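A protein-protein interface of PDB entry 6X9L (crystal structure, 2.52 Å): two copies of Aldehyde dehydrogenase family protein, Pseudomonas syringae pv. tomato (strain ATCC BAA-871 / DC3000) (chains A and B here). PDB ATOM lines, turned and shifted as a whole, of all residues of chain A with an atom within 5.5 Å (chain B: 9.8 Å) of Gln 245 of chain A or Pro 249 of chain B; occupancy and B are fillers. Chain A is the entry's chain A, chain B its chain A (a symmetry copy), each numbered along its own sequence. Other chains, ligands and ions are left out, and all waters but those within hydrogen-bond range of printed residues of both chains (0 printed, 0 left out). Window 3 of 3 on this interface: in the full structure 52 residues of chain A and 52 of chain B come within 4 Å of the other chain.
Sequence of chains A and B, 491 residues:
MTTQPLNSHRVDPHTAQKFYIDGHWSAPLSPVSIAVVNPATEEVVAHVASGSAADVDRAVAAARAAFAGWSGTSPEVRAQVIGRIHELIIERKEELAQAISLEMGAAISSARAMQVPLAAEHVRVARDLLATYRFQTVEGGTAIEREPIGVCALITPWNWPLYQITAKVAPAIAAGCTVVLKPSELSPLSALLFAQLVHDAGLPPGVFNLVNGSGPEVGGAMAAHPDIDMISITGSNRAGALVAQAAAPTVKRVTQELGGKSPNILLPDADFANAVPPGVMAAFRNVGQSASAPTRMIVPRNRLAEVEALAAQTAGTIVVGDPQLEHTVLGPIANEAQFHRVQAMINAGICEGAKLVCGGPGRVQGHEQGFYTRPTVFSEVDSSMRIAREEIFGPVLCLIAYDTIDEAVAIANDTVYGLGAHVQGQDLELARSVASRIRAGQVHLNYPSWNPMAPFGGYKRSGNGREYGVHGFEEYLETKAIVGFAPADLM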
ATOM      1  N   GLY A 240       5.791  -8.026 -11.708  1.00  0.00           N
ATOM      2  CA  GLY A 240       5.327  -7.208 -10.600  1.00  0.00           C
ATOM      3  C   GLY A 240       4.055  -7.748  -9.980  1.00  0.00           C
ATOM      4  O   GLY A 240       3.912  -7.793  -8.754  1.00  0.00           O
ATOM      5  N   ALA A 241       3.109  -8.159 -10.817  1.00  0.00           N
ATOM      6  CA  ALA A 241       1.832  -8.628 -10.296  1.00  0.00           C
ATOM      7  C   ALA A 241       1.985  -9.979  -9.602  1.00  0.00           C
ATOM      8  O   ALA A 241       1.386 -10.205  -8.541  1.00  0.00           O
ATOM      9  CB  ALA A 241       0.796  -8.697 -11.423  1.00  0.00           C
ATOM     10  N   LEU A 242       2.803 -10.881 -10.173  1.00  0.00           N
ATOM     11  CA  LEU A 242       3.053 -12.172  -9.528  1.00  0.00           C
ATOM     12  C   LEU A 242       3.690 -12.003  -8.157  1.00  0.00           C
ATOM     13  O   LEU A 242       3.337 -12.725  -7.212  1.00  0.00           O
ATOM     14  CB  LEU A 242       3.940 -13.051 -10.391  1.00  0.00           C
ATOM     15  CG  LEU A 242       3.333 -13.507 -11.703  1.00  0.00           C
ATOM     16  CD1 LEU A 242       4.421 -14.249 -12.452  1.00  0.00           C
ATOM     17  CD2 LEU A 242       2.090 -14.379 -11.465  1.00  0.00           C
ATOM     18  N   VAL A 243       4.624 -11.061  -8.012  1.00  0.00           N
ATOM     19  CA  VAL A 243       5.170 -10.859  -6.674  1.00  0.00           C
ATOM     20  C   VAL A 243       4.095 -10.277  -5.750  1.00  0.00           C
ATOM     21  O   VAL A 243       3.941 -10.725  -4.606  1.00  0.00           O
ATOM     22  CB  VAL A 243       6.464 -10.007  -6.679  1.00  0.00           C
ATOM     23  CG1 VAL A 243       7.006  -9.802  -8.057  1.00  0.00           C
ATOM     24  CG2 VAL A 243       6.264  -8.685  -5.984  1.00  0.00           C
ATOM     25  N   ALA A 244       3.304  -9.308  -6.231  1.00  0.00           N
ATOM     26  CA  ALA A 244       2.223  -8.783  -5.397  1.00  0.00           C
ATOM     27  C   ALA A 244       1.319  -9.907  -4.903  1.00  0.00           C
ATOM     28  O   ALA A 244       1.003  -9.993  -3.708  1.00  0.00           O
ATOM     29  CB  ALA A 244       1.406  -7.752  -6.167  1.00  0.00           C
ATOM     30  N   GLN A 245       0.895 -10.783  -5.819  1.00  0.00           N
ATOM     31  CA  GLN A 245       0.037 -11.905  -5.453  1.00  0.00           C
ATOM     32  C   GLN A 245       0.733 -12.854  -4.491  1.00  0.00           C
ATOM     33  O   GLN A 245       0.111 -13.339  -3.541  1.00  0.00           O
ATOM     34  CB  GLN A 245      -0.401 -12.665  -6.704  1.00  0.00           C
ATOM     35  CG  GLN A 245      -1.611 -12.069  -7.375  1.00  0.00           C
ATOM     36  CD  GLN A 245      -1.672 -12.390  -8.853  1.00  0.00           C
ATOM     37  OE1 GLN A 245      -0.828 -13.127  -9.372  1.00  0.00           O
ATOM     38  NE2 GLN A 245      -2.670 -11.833  -9.541  1.00  0.00           N
ATOM     39  N   ALA A 246       2.019 -13.136  -4.723  1.00  0.00           N
ATOM     40  CA  ALA A 246       2.735 -14.046  -3.833  1.00  0.00           C
ATOM     41  C   ALA A 246       2.886 -13.456  -2.442  1.00  0.00           C
ATOM     42  O   ALA A 246       2.887 -14.205  -1.455  1.00  0.00           O
ATOM     43  CB  ALA A 246       4.112 -14.401  -4.410  1.00  0.00           C
ATOM     44  N   ALA A 247       2.983 -12.120  -2.347  1.00  0.00           N
ATOM     45  CA  ALA A 247       3.211 -11.407  -1.093  1.00  0.00           C
ATOM     46  C   ALA A 247       1.946 -11.136  -0.287  1.00  0.00           C
ATOM     47  O   ALA A 247       2.043 -10.849   0.905  1.00  0.00           O
ATOM     48  CB  ALA A 247       3.895 -10.072  -1.376  1.00  0.00           C
ATOM     49  N   ALA A 248       0.770 -11.213  -0.900  1.00  0.00           N
ATOM     50  CA  ALA A 248      -0.450 -10.805  -0.207  1.00  0.00           C
ATOM     51  C   ALA A 248      -0.665 -11.532   1.114  1.00  0.00           C
ATOM     52  O   ALA A 248      -0.934 -10.864   2.125  1.00  0.00           O
ATOM     53  CB  ALA A 248      -1.658 -10.983  -1.143  1.00  0.00           C
ATOM     54  N   PRO A 249      -0.569 -12.863   1.198  1.00  0.00           N
ATOM     55  CA  PRO A 249      -0.938 -13.527   2.468  1.00  0.00           C
ATOM     56  C   PRO A 249      -0.047 -13.154   3.649  1.00  0.00           C
ATOM     57  O   PRO A 249      -0.523 -13.198   4.788  1.00  0.00           O
ATOM     58  CB  PRO A 249      -0.873 -15.022   2.126  1.00  0.00           C
ATOM     59  CG  PRO A 249      -0.147 -15.108   0.836  1.00  0.00           C
ATOM     60  CD  PRO A 249      -0.253 -13.818   0.117  1.00  0.00           C
ATOM     61  N   ARG A 461      -0.620   1.938 -13.900  1.00  0.00           N
ATOM     62  CA  ARG A 461      -0.001   0.624 -13.959  1.00  0.00           C
ATOM     63  C   ARG A 461       1.516   0.652 -14.112  1.00  0.00           C
ATOM     64  O   ARG A 461       2.100  -0.386 -14.427  1.00  0.00           O
ATOM     65  CB  ARG A 461      -0.611  -0.177 -15.102  1.00  0.00           C
ATOM     66  CG  ARG A 461      -2.038  -0.519 -14.845  1.00  0.00           C
ATOM     67  CD  ARG A 461      -2.484  -1.594 -15.752  1.00  0.00           C
ATOM     68  NE  ARG A 461      -3.925  -1.529 -15.940  1.00  0.00           N
ATOM     69  CZ  ARG A 461      -4.586  -2.341 -16.753  1.00  0.00           C
ATOM     70  NH1 ARG A 461      -3.917  -3.266 -17.428  1.00  0.00           N
ATOM     71  NH2 ARG A 461      -5.898  -2.230 -16.886  1.00  0.00           N
ATOM     72  N   GLY B 220     -15.267  -8.054  -4.573  1.00  0.00           N
ATOM     73  CA  GLY B 220     -14.425  -8.671  -5.584  1.00  0.00           C
ATOM     74  C   GLY B 220     -14.443  -7.898  -6.889  1.00  0.00           C
ATOM     75  O   GLY B 220     -13.391  -7.664  -7.504  1.00  0.00           O
ATOM     76  N   ALA B 223     -12.229  -4.824  -6.413  1.00  0.00           N
ATOM     77  CA  ALA B 223     -10.798  -5.116  -6.378  1.00  0.00           C
ATOM     78  C   ALA B 223     -10.249  -5.371  -7.773  1.00  0.00           C
ATOM     79  O   ALA B 223      -9.083  -5.053  -8.051  1.00  0.00           O
ATOM     80  CB  ALA B 223     -10.525  -6.314  -5.464  1.00  0.00           C
ATOM     81  N   ALA B 224     -11.076  -5.914  -8.665  1.00  0.00           N
ATOM     82  CA  ALA B 224     -10.651  -6.282 -10.006  1.00  0.00           C
ATOM     83  C   ALA B 224     -11.010  -5.260 -11.073  1.00  0.00           C
ATOM     84  O   ALA B 224     -10.685  -5.476 -12.245  1.00  0.00           O
ATOM     85  CB  ALA B 224     -11.255  -7.632 -10.398  1.00  0.00           C
ATOM     86  N   HIS B 225     -11.657  -4.166 -10.725  1.00  0.00           N
ATOM     87  CA  HIS B 225     -12.202  -3.312 -11.766  1.00  0.00           C
ATOM     88  C   HIS B 225     -11.081  -2.589 -12.505  1.00  0.00           C
ATOM     89  O   HIS B 225     -10.191  -2.008 -11.873  1.00  0.00           O
ATOM     90  CB  HIS B 225     -13.193  -2.316 -11.188  1.00  0.00           C
ATOM     91  CG  HIS B 225     -14.097  -1.717 -12.218  1.00  0.00           C
ATOM     92  ND1 HIS B 225     -13.643  -0.837 -13.176  1.00  0.00           N
ATOM     93  CD2 HIS B 225     -15.425  -1.873 -12.446  1.00  0.00           C
ATOM     94  CE1 HIS B 225     -14.649  -0.481 -13.957  1.00  0.00           C
ATOM     95  NE2 HIS B 225     -15.744  -1.091 -13.533  1.00  0.00           N
ATOM     96  N   PRO B 226     -11.097  -2.585 -13.837  1.00  0.00           N
ATOM     97  CA  PRO B 226     -10.025  -1.921 -14.598  1.00  0.00           C
ATOM     98  C   PRO B 226     -10.029  -0.402 -14.495  1.00  0.00           C
ATOM     99  O   PRO B 226      -9.072   0.239 -14.954  1.00  0.00           O
ATOM    100  CB  PRO B 226     -10.297  -2.358 -16.045  1.00  0.00           C
ATOM    101  CG  PRO B 226     -11.572  -3.162 -16.019  1.00  0.00           C
ATOM    102  CD  PRO B 226     -12.201  -3.045 -14.694  1.00  0.00           C
ATOM    103  N   ILE B 228     -10.689   1.393 -11.550  1.00  0.00           N
ATOM    104  CA  ILE B 228     -10.497   1.836 -10.175  1.00  0.00           C
ATOM    105  C   ILE B 228      -9.004   1.972  -9.921  1.00  0.00           C
ATOM    106  O   ILE B 228      -8.231   1.040 -10.158  1.00  0.00           O
ATOM    107  CB  ILE B 228     -11.166   0.865  -9.188  1.00  0.00           C
ATOM    108  CG1 ILE B 228     -12.679   1.011  -9.351  1.00  0.00           C
ATOM    109  CG2 ILE B 228     -10.680   1.111  -7.755  1.00  0.00           C
ATOM    110  CD1 ILE B 228     -13.516   0.225  -8.384  1.00  0.00           C
ATOM    111  N   GLY B 240      -8.503  -9.038   3.393  1.00  0.00           N
ATOM    112  CA  GLY B 240      -7.472  -8.121   2.939  1.00  0.00           C
ATOM    113  C   GLY B 240      -6.578  -8.738   1.883  1.00  0.00           C
ATOM    114  O   GLY B 240      -6.241  -8.100   0.880  1.00  0.00           O
ATOM    115  N   ALA B 241      -6.176  -9.986   2.096  1.00  0.00           N
ATOM    116  CA  ALA B 241      -5.260 -10.623   1.158  1.00  0.00           C
ATOM    117  C   ALA B 241      -5.958 -10.936  -0.163  1.00  0.00           C
ATOM    118  O   ALA B 241      -5.371 -10.745  -1.238  1.00  0.00           O
ATOM    119  CB  ALA B 241      -4.660 -11.887   1.782  1.00  0.00           C
ATOM    120  N   LEU B 242      -7.221 -11.394  -0.106  1.00  0.00           N
ATOM    121  CA  LEU B 242      -7.977 -11.649  -1.333  1.00  0.00           C
ATOM    122  C   LEU B 242      -8.146 -10.387  -2.165  1.00  0.00           C
ATOM    123  O   LEU B 242      -8.045 -10.436  -3.400  1.00  0.00           O
ATOM    124  CB  LEU B 242      -9.344 -12.233  -1.022  1.00  0.00           C
ATOM    125  CG  LEU B 242      -9.338 -13.617  -0.403  1.00  0.00           C
ATOM    126  CD1 LEU B 242     -10.777 -13.945  -0.057  1.00  0.00           C
ATOM    127  CD2 LEU B 242      -8.719 -14.649  -1.359  1.00  0.00           C
ATOM    128  N   VAL B 243      -8.397  -9.244  -1.524  1.00  0.00           N
ATOM    129  CA  VAL B 243      -8.480  -8.030  -2.328  1.00  0.00           C
ATOM    130  C   VAL B 243      -7.101  -7.685  -2.903  1.00  0.00           C
ATOM    131  O   VAL B 243      -6.983  -7.345  -4.087  1.00  0.00           O
ATOM    132  CB  VAL B 243      -9.106  -6.842  -1.554  1.00  0.00           C
ATOM    133  CG1 VAL B 243      -9.719  -7.266  -0.259  1.00  0.00           C
ATOM    134  CG2 VAL B 243      -8.109  -5.733  -1.333  1.00  0.00           C
ATOM    135  N   ALA B 244      -6.033  -7.807  -2.103  1.00  0.00           N
ATOM    136  CA  ALA B 244      -4.698  -7.556  -2.644  1.00  0.00           C
ATOM    137  C   ALA B 244      -4.441  -8.406  -3.882  1.00  0.00           C
ATOM    138  O   ALA B 244      -3.988  -7.903  -4.920  1.00  0.00           O
ATOM    139  CB  ALA B 244      -3.632  -7.829  -1.588  1.00  0.00           C
ATOM    140  N   GLN B 245      -4.729  -9.707  -3.787  1.00  0.00           N
ATOM    141  CA  GLN B 245      -4.534 -10.611  -4.916  1.00  0.00           C
ATOM    142  C   GLN B 245      -5.418 -10.236  -6.095  1.00  0.00           C
ATOM    143  O   GLN B 245      -4.969 -10.281  -7.244  1.00  0.00           O
ATOM    144  CB  GLN B 245      -4.817 -12.052  -4.495  1.00  0.00           C
ATOM    145  CG  GLN B 245      -3.634 -12.733  -3.855  1.00  0.00           C
ATOM    146  CD  GLN B 245      -4.044 -13.850  -2.920  1.00  0.00           C
ATOM    147  OE1 GLN B 245      -5.232 -14.164  -2.796  1.00  0.00           O
ATOM    148  NE2 GLN B 245      -3.061 -14.453  -2.249  1.00  0.00           N
ATOM    149  N   ALA B 246      -6.677  -9.872  -5.831  1.00  0.00           N
ATOM    150  CA  ALA B 246      -7.571  -9.507  -6.927  1.00  0.00           C
ATOM    151  C   ALA B 246      -7.112  -8.234  -7.615  1.00  0.00           C
ATOM    152  O   ALA B 246      -7.311  -8.088  -8.830  1.00  0.00           O
ATOM    153  CB  ALA B 246      -9.012  -9.346  -6.423  1.00  0.00           C
ATOM    154  N   ALA B 247      -6.474  -7.322  -6.864  1.00  0.00           N
ATOM    155  CA  ALA B 247      -6.041  -6.018  -7.358  1.00  0.00           C
ATOM    156  C   ALA B 247      -4.693  -6.031  -8.067  1.00  0.00           C
ATOM    157  O   ALA B 247      -4.386  -5.089  -8.795  1.00  0.00           O
ATOM    158  CB  ALA B 247      -5.963  -5.028  -6.198  1.00  0.00           C
ATOM    159  N   ALA B 248      -3.880  -7.064  -7.871  1.00  0.00           N
ATOM    160  CA  ALA B 248      -2.518  -7.040  -8.402  1.00  0.00           C
ATOM    161  C   ALA B 248      -2.459  -6.793  -9.903  1.00  0.00           C
ATOM    162  O   ALA B 248      -1.686  -5.923 -10.335  1.00  0.00           O
ATOM    163  CB  ALA B 248      -1.795  -8.344  -8.025  1.00  0.00           C
ATOM    164  N   PRO B 249      -3.221  -7.492 -10.752  1.00  0.00           N
ATOM    165  CA  PRO B 249      -3.012  -7.318 -12.207  1.00  0.00           C
ATOM    166  C   PRO B 249      -3.321  -5.914 -12.719  1.00  0.00           C
ATOM    167  O   PRO B 249      -2.724  -5.503 -13.719  1.00  0.00           O
ATOM    168  CB  PRO B 249      -3.917  -8.389 -12.832  1.00  0.00           C
ATOM    169  CG  PRO B 249      -4.818  -8.838 -11.744  1.00  0.00           C
ATOM    170  CD  PRO B 249      -4.196  -8.552 -10.431  1.00  0.00           C
ATOM    171  N   THR B 250      -4.179  -5.136 -12.048  1.00  0.00           N
ATOM    172  CA  THR B 250      -4.365  -3.742 -12.442  1.00  0.00           C
ATOM    173  C   THR B 250      -3.430  -2.769 -11.725  1.00  0.00           C
ATOM    174  O   THR B 250      -3.447  -1.573 -12.041  1.00  0.00           O
ATOM    175  CB  THR B 250      -5.804  -3.329 -12.199  1.00  0.00           C
ATOM    176  OG1 THR B 250      -6.196  -3.794 -10.909  1.00  0.00           O
ATOM    177  CG2 THR B 250      -6.702  -3.947 -13.257  1.00  0.00           C
ATOM    178  N   VAL B 251      -2.625  -3.249 -10.772  1.00  0.00           N
ATOM    179  CA  VAL B 251      -1.572  -2.467 -10.132  1.00  0.00           C
ATOM    180  C   VAL B 251      -2.178  -1.297  -9.371  1.00  0.00           C
ATOM    181  O   VAL B 251      -1.588  -0.206  -9.307  1.00  0.00           O
ATOM    182  CB  VAL B 251      -0.525  -1.984 -11.155  1.00  0.00           C
ATOM    183  CG1 VAL B 251       0.759  -1.480 -10.445  1.00  0.00           C
ATOM    184  CG2 VAL B 251      -0.199  -3.101 -12.094  1.00  0.00           C
ATOM    185  N   LYS B 252      -3.344  -1.520  -8.764  1.00  0.00           N
ATOM    186  CA  LYS B 252      -3.936  -0.479  -7.937  1.00  0.00           C
ATOM    187  C   LYS B 252      -3.072  -0.202  -6.717  1.00  0.00           C
ATOM    188  O   LYS B 252      -2.251  -1.028  -6.307  1.00  0.00           O
ATOM    189  CB  LYS B 252      -5.330  -0.873  -7.465  1.00  0.00           C
ATOM    190  CG  LYS B 252      -6.034  -1.805  -8.377  1.00  0.00           C
ATOM    191  CD  LYS B 252      -7.528  -1.710  -8.178  1.00  0.00           C
ATOM    192  CE  LYS B 252      -8.234  -2.455  -9.274  1.00  0.00           C
ATOM    193  NZ  LYS B 252      -9.570  -1.924  -9.360  1.00  0.00           N
ATOM    194  N   ARG B 253      -3.251   0.998  -6.160  1.00  0.00           N
ATOM    195  CA  ARG B 253      -2.826   1.278  -4.796  1.00  0.00           C
ATOM    196  C   ARG B 253      -3.749   0.552  -3.827  1.00  0.00           C
ATOM    197  O   ARG B 253      -4.976   0.670  -3.917  1.00  0.00           O
ATOM    198  CB  ARG B 253      -2.852   2.774  -4.483  1.00  0.00           C
ATOM    199  CG  ARG B 253      -2.557   3.028  -2.998  1.00  0.00           C
ATOM    200  CD  ARG B 253      -2.268   4.488  -2.702  1.00  0.00           C
ATOM    201  NE  ARG B 253      -1.174   5.004  -3.522  1.00  0.00           N
ATOM    202  CZ  ARG B 253      -0.862   6.289  -3.607  1.00  0.00           C
ATOM    203  NH1 ARG B 253      -1.567   7.183  -2.932  1.00  0.00           N
ATOM    204  NH2 ARG B 253       0.137   6.677  -4.376  1.00  0.00           N
ATOM    205  N   VAL B 254      -3.151  -0.212  -2.919  1.00  0.00           N
ATOM    206  CA  VAL B 254      -3.871  -1.082  -2.001  1.00  0.00           C
ATOM    207  C   VAL B 254      -3.612  -0.576  -0.589  1.00  0.00           C
ATOM    208  O   VAL B 254      -2.457  -0.515  -0.142  1.00  0.00           O
ATOM    209  CB  VAL B 254      -3.432  -2.552  -2.156  1.00  0.00           C
ATOM    210  CG1 VAL B 254      -4.010  -3.426  -1.024  1.00  0.00           C
ATOM    211  CG2 VAL B 254      -3.819  -3.093  -3.553  1.00  0.00           C
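O of Ala 247 of chain B is in hydrogen-bond range of OG1 of Thr 250 of chain B, at 3.1 Å.
Among the printed residues, pairs that only touch across the chains: Arg 461 of chain A with Thr 250 of chain B, Gln 245 of chain A with Gln 245 of chain B, Ala 241 of chain A with Ala 248 of chain B, Ala 248 of chain A with Ala 241 of chain B, Gln 245 of chain A with Pro 249 of chain B, Pro 249 of chain A with Gln 245 of chain B, Ala 248 of chain A with Ala 244 of chain B, Ala 244 of chain A with Ala 248 of chain B, Ala 248 of chain A with Gln 245 of chain B, Gln 245 of chain A with Ala 248 of chain B and Arg 461 of chain A with Val 251 of chain B.
Of the 21 printed residues of chain B, 7 touch a printed residue of chain A.
Printed residues of chain A that touch a printed residue of chain B: Ala 241, Ala 244, Gln 245, Ala 248, Pro 249 and Arg 461.
Hydrophobic or aromatic side chains of chain A within 4 Å of the printed part of chain B: Ala 241, Ala 244, Ala 248 and Pro 249.
Among the printed residues, 11 pairs touch across the chains.
Among the printed residues, no Asp or Glu carboxylate lies within 4 Å of a Lys or Arg side-chain nitrogen of the other chain.
Of the printed residues of chain B, Ala 241 of chain A touches Ala 248 (3.7 Å).
Gln 245 of chain A touches just these residues of chain B: Gln 245 (3.6 Å), Ala 248 (3.8 Å) and Pro 249 (3.7 Å).
Ala 246 of chain A touches none of the printed residues of chain B.
Printed residues of chain B within 4 Å of Pro 249 of chain A: Gln 245 (3.7 Å).
Printed residues of chain A within 4 Å of Gln 245 of chain B: Gln 245, Ala 248 and Pro 249.
Printed residues of chain A within 4 Å of Ala 248 of chain B: Ala 241 (3.7 Å), Ala 244 (3.7 Å) and Gln 245 (3.8 Å).
Pro 249 of chain B touches just one residue of chain A: Gln 245.
Of the printed residues of chain A, Thr 250 of chain B touches Arg 461 (3.3 Å).
Lys 252 of chain B touches none of the printed residues of chain A.
The nearest residue of chain A that does not touch Pro 249 of chain B is Ala 241 of chain A (4.1 Å).
Ala 241 of chain A touches Ala 248 of chain B, and with the chains exchanged Ala 248 of chain A touches Ala 241 of chain B.
Ala 244 of chain A touches Ala 248 of chain B, and with the chains exchanged Ala 248 of chain A touches Ala 244 of chain B.
Gln 245 of chain B touches its own counterpart, Gln 245 of chain A.
Gln 245 of chain A touches Pro 249 of chain B, and with the chains exchanged Pro 249 of chain A touches Gln 245 of chain B.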
